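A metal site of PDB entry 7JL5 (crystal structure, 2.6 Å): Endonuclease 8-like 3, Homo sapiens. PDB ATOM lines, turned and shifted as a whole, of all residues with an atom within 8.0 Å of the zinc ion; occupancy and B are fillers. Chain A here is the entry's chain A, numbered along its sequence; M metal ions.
The zinc ion is bound by ND1 of His 59 (2.2 Å), SG of Cys 82 (2.3 Å), SG of Cys 57 (2.4 Å) and SG of Cys 90 (2.4 Å).
N of Asn 58 lies close to SG of Cys 90.
The backbone NH (N) of Phe 92 lies close to the side-chain sulfur (SG) of Cys 90 (3.5 Å).
O of Cys 82 is in hydrogen-bond range of NE2 of Gln 89.
The backbone carbonyl oxygen (O) of Lys 61 sits close to the side-chain sulfur (SG) of Cys 57 (3.6 Å).
Four residues have an atom within 4 Å of the zinc ion: Cys 57, His 59, Cys 82 and Cys 90.
The nearest printed residue that does not touch the zinc ion is Asn 58 (4.02 Å).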
ATOM      1  N   PHE A  56      -3.063 -16.829   7.820  1.00  0.00           N
ATOM      2  CA  PHE A  56      -3.647 -15.567   8.230  1.00  0.00           C
ATOM      3  C   PHE A  56      -2.710 -14.426   7.828  1.00  0.00           C
ATOM      4  O   PHE A  56      -1.501 -14.510   8.068  1.00  0.00           O
ATOM      5  CB  PHE A  56      -3.891 -15.533   9.743  1.00  0.00           C
ATOM      6  CG  PHE A  56      -4.892 -16.539  10.212  1.00  0.00           C
ATOM      7  CD1 PHE A  56      -6.247 -16.224  10.262  1.00  0.00           C
ATOM      8  CD2 PHE A  56      -4.495 -17.805  10.617  1.00  0.00           C
ATOM      9  CE1 PHE A  56      -7.164 -17.143  10.699  1.00  0.00           C
ATOM     10  CE2 PHE A  56      -5.421 -18.735  11.054  1.00  0.00           C
ATOM     11  CZ  PHE A  56      -6.760 -18.405  11.098  1.00  0.00           C
ATOM     12  N   CYS A  57      -3.268 -13.386   7.219  1.00  0.00           N
ATOM     13  CA  CYS A  57      -2.475 -12.211   6.898  1.00  0.00           C
ATOM     14  C   CYS A  57      -2.183 -11.425   8.169  1.00  0.00           C
ATOM     15  O   CYS A  57      -2.603 -11.790   9.278  1.00  0.00           O
ATOM     16  CB  CYS A  57      -3.196 -11.350   5.863  1.00  0.00           C
ATOM     17  SG  CYS A  57      -4.560 -10.357   6.503  1.00  0.00           S
ATOM     18  N   ASN A  58      -1.462 -10.316   8.021  1.00  0.00           N
ATOM     19  CA  ASN A  58      -1.034  -9.557   9.190  1.00  0.00           C
ATOM     20  C   ASN A  58      -2.177  -8.806   9.853  1.00  0.00           C
ATOM     21  O   ASN A  58      -1.984  -8.282  10.957  1.00  0.00           O
ATOM     22  CB  ASN A  58       0.075  -8.587   8.776  1.00  0.00           C
ATOM     23  CG  ASN A  58       1.355  -9.308   8.407  1.00  0.00           C
ATOM     24  OD1 ASN A  58       1.859  -9.161   7.289  1.00  0.00           O
ATOM     25  ND2 ASN A  58       1.889 -10.099   9.327  1.00  0.00           N
ATOM     26  N   HIS A  59      -3.349  -8.729   9.224  1.00  0.00           N
ATOM     27  CA  HIS A  59      -4.527  -8.179   9.880  1.00  0.00           C
ATOM     28  C   HIS A  59      -5.177  -9.168  10.839  1.00  0.00           C
ATOM     29  O   HIS A  59      -6.049  -8.769  11.620  1.00  0.00           O
ATOM     30  CB  HIS A  59      -5.572  -7.749   8.859  1.00  0.00           C
ATOM     31  CG  HIS A  59      -5.261  -6.458   8.168  1.00  0.00           C
ATOM     32  ND1 HIS A  59      -4.855  -6.387   6.857  1.00  0.00           N
ATOM     33  CD2 HIS A  59      -5.326  -5.173   8.611  1.00  0.00           C
ATOM     34  CE1 HIS A  59      -4.677  -5.128   6.517  1.00  0.00           C
ATOM     35  NE2 HIS A  59      -4.946  -4.369   7.572  1.00  0.00           N
ATOM     36  N   GLY A  60      -4.799 -10.436  10.791  1.00  0.00           N
ATOM     37  CA  GLY A  60      -5.510 -11.483  11.481  1.00  0.00           C
ATOM     38  C   GLY A  60      -6.619 -12.118  10.684  1.00  0.00           C
ATOM     39  O   GLY A  60      -7.378 -12.935  11.235  1.00  0.00           O
ATOM     40  N   LYS A  61      -6.743 -11.788   9.408  1.00  0.00           N
ATOM     41  CA  LYS A  61      -7.802 -12.286   8.535  1.00  0.00           C
ATOM     42  C   LYS A  61      -7.266 -13.404   7.638  1.00  0.00           C
ATOM     43  O   LYS A  61      -6.069 -13.485   7.355  1.00  0.00           O
ATOM     44  CB  LYS A  61      -8.372 -11.162   7.680  1.00  0.00           C
ATOM     45  CG  LYS A  61      -9.067 -10.082   8.499  1.00  0.00           C
ATOM     46  CD  LYS A  61      -9.432  -8.863   7.660  1.00  0.00           C
ATOM     47  CE  LYS A  61     -10.412  -7.976   8.412  1.00  0.00           C
ATOM     48  NZ  LYS A  61     -10.454  -6.580   7.892  1.00  0.00           N
ATOM     49  N   ARG A  62      -8.175 -14.277   7.205  1.00  0.00           N
ATOM     50  CA  ARG A  62      -7.805 -15.348   6.304  1.00  0.00           C
ATOM     51  C   ARG A  62      -7.292 -14.776   4.994  1.00  0.00           C
ATOM     52  O   ARG A  62      -7.932 -13.917   4.384  1.00  0.00           O
ATOM     53  CB  ARG A  62      -8.993 -16.270   6.041  1.00  0.00           C
ATOM     54  CG  ARG A  62      -9.345 -17.194   7.192  1.00  0.00           C
ATOM     55  CD  ARG A  62      -8.389 -18.372   7.284  1.00  0.00           C
ATOM     56  NE  ARG A  62      -8.813 -19.314   8.323  1.00  0.00           N
ATOM     57  CZ  ARG A  62      -8.037 -20.255   8.848  1.00  0.00           C
ATOM     58  NH1 ARG A  62      -6.786 -20.404   8.441  1.00  0.00           N
ATOM     59  NH2 ARG A  62      -8.527 -21.055   9.792  1.00  0.00           N
ATOM     60  N   SER A  63      -6.130 -15.256   4.558  1.00  0.00           N
ATOM     61  CA  SER A  63      -5.562 -14.778   3.308  1.00  0.00           C
ATOM     62  C   SER A  63      -6.332 -15.332   2.117  1.00  0.00           C
ATOM     63  O   SER A  63      -7.117 -16.284   2.230  1.00  0.00           O
ATOM     64  CB  SER A  63      -4.081 -15.171   3.215  1.00  0.00           C
ATOM     65  OG  SER A  63      -3.905 -16.549   3.475  1.00  0.00           O
ATOM     66  N   VAL A  81      -2.171 -13.817  -0.106  1.00  0.00           N
ATOM     67  CA  VAL A  81      -2.071 -12.373   0.078  1.00  0.00           C
ATOM     68  C   VAL A  81      -3.207 -11.897   0.973  1.00  0.00           C
ATOM     69  O   VAL A  81      -4.136 -12.634   1.286  1.00  0.00           O
ATOM     70  CB  VAL A  81      -2.100 -11.612  -1.268  1.00  0.00           C
ATOM     71  CG1 VAL A  81      -0.889 -11.978  -2.109  1.00  0.00           C
ATOM     72  CG2 VAL A  81      -3.391 -11.911  -2.005  1.00  0.00           C
ATOM     73  N   CYS A  82      -3.107 -10.637   1.381  1.00  0.00           N
ATOM     74  CA  CYS A  82      -4.172 -10.003   2.153  1.00  0.00           C
ATOM     75  C   CYS A  82      -5.447  -9.740   1.344  1.00  0.00           C
ATOM     76  O   CYS A  82      -5.374  -9.248   0.227  1.00  0.00           O
ATOM     77  CB  CYS A  82      -3.720  -8.627   2.631  1.00  0.00           C
ATOM     78  SG  CYS A  82      -4.879  -7.769   3.716  1.00  0.00           S
ATOM     79  N   PRO A  83      -6.612 -10.175   1.863  1.00  0.00           N
ATOM     80  CA  PRO A  83      -7.843 -10.070   1.050  1.00  0.00           C
ATOM     81  C   PRO A  83      -8.646  -8.784   1.068  1.00  0.00           C
ATOM     82  O   PRO A  83      -9.881  -8.850   0.959  1.00  0.00           O
ATOM     83  CB  PRO A  83      -8.655 -11.213   1.680  1.00  0.00           C
ATOM     84  CG  PRO A  83      -8.370 -11.013   3.153  1.00  0.00           C
ATOM     85  CD  PRO A  83      -6.899 -10.598   3.228  1.00  0.00           C
ATOM     86  N   LEU A  84      -8.009  -7.624   1.196  1.00  0.00           N
ATOM     87  CA  LEU A  84      -8.740  -6.401   1.510  1.00  0.00           C
ATOM     88  C   LEU A  84      -8.784  -5.368   0.400  1.00  0.00           C
ATOM     89  O   LEU A  84      -9.535  -4.389   0.518  1.00  0.00           O
ATOM     90  CB  LEU A  84      -8.156  -5.750   2.768  1.00  0.00           C
ATOM     91  CG  LEU A  84      -8.560  -6.342   4.113  1.00  0.00           C
ATOM     92  CD1 LEU A  84      -8.097  -5.435   5.243  1.00  0.00           C
ATOM     93  CD2 LEU A  84     -10.062  -6.569   4.190  1.00  0.00           C
ATOM     94  N   LYS A  88      -5.843  -0.999   1.039  1.00  0.00           N
ATOM     95  CA  LYS A  88      -5.806  -1.335   2.456  1.00  0.00           C
ATOM     96  C   LYS A  88      -5.146  -2.679   2.748  1.00  0.00           C
ATOM     97  O   LYS A  88      -5.199  -3.151   3.883  1.00  0.00           O
ATOM     98  CB  LYS A  88      -7.230  -1.334   3.036  1.00  0.00           C
ATOM     99  N   GLN A  89      -4.523  -3.302   1.742  1.00  0.00           N
ATOM    100  CA  GLN A  89      -3.851  -4.570   1.959  1.00  0.00           C
ATOM    101  C   GLN A  89      -2.687  -4.405   2.931  1.00  0.00           C
ATOM    102  O   GLN A  89      -1.970  -3.398   2.901  1.00  0.00           O
ATOM    103  CB  GLN A  89      -3.324  -5.137   0.641  1.00  0.00           C
ATOM    104  CG  GLN A  89      -4.327  -5.963  -0.140  1.00  0.00           C
ATOM    105  CD  GLN A  89      -3.670  -6.721  -1.281  1.00  0.00           C
ATOM    106  OE1 GLN A  89      -3.455  -6.175  -2.364  1.00  0.00           O
ATOM    107  NE2 GLN A  89      -3.325  -7.983  -1.035  1.00  0.00           N
ATOM    108  N   CYS A  90      -2.490  -5.400   3.798  1.00  0.00           N
ATOM    109  CA  CYS A  90      -1.262  -5.493   4.567  1.00  0.00           C
ATOM    110  C   CYS A  90      -0.161  -6.022   3.634  1.00  0.00           C
ATOM    111  O   CYS A  90      -0.353  -6.136   2.419  1.00  0.00           O
ATOM    112  CB  CYS A  90      -1.454  -6.378   5.796  1.00  0.00           C
ATOM    113  SG  CYS A  90      -1.624  -8.137   5.465  1.00  0.00           S
ATOM    114  N   ASN A  91       0.988  -6.364   4.200  1.00  0.00           N
ATOM    115  CA  ASN A  91       2.147  -6.772   3.405  1.00  0.00           C
ATOM    116  C   ASN A  91       2.374  -8.276   3.407  1.00  0.00           C
ATOM    117  O   ASN A  91       3.443  -8.725   2.994  1.00  0.00           O
ATOM    118  CB  ASN A  91       3.393  -6.047   3.921  1.00  0.00           C
ATOM    119  CG  ASN A  91       3.787  -6.480   5.324  1.00  0.00           C
ATOM    120  OD1 ASN A  91       3.078  -6.209   6.292  1.00  0.00           O
ATOM    121  ND2 ASN A  91       4.922  -7.163   5.433  1.00  0.00           N
ATOM    122  N   PHE A  92       1.393  -9.058   3.848  1.00  0.00           N
ATOM    123  CA  PHE A  92       1.571 -10.498   3.961  1.00  0.00           C
ATOM    124  C   PHE A  92       1.696 -11.141   2.588  1.00  0.00           C
ATOM    125  O   PHE A  92       0.930 -10.829   1.664  1.00  0.00           O
ATOM    126  CB  PHE A  92       0.388 -11.104   4.725  1.00  0.00           C
ATOM    127  CG  PHE A  92       0.402 -12.615   4.768  1.00  0.00           C
ATOM    128  CD1 PHE A  92       1.245 -13.285   5.627  1.00  0.00           C
ATOM    129  CD2 PHE A  92      -0.440 -13.354   3.948  1.00  0.00           C
ATOM    130  CE1 PHE A  92       1.258 -14.676   5.673  1.00  0.00           C
ATOM    131  CE2 PHE A  92      -0.433 -14.730   3.978  1.00  0.00           C
ATOM    132  CZ  PHE A  92       0.419 -15.398   4.848  1.00  0.00           C
HETATM  133 ZN    ZN M   1      -4.044  -8.166   5.808  1.00  0.00          ZN
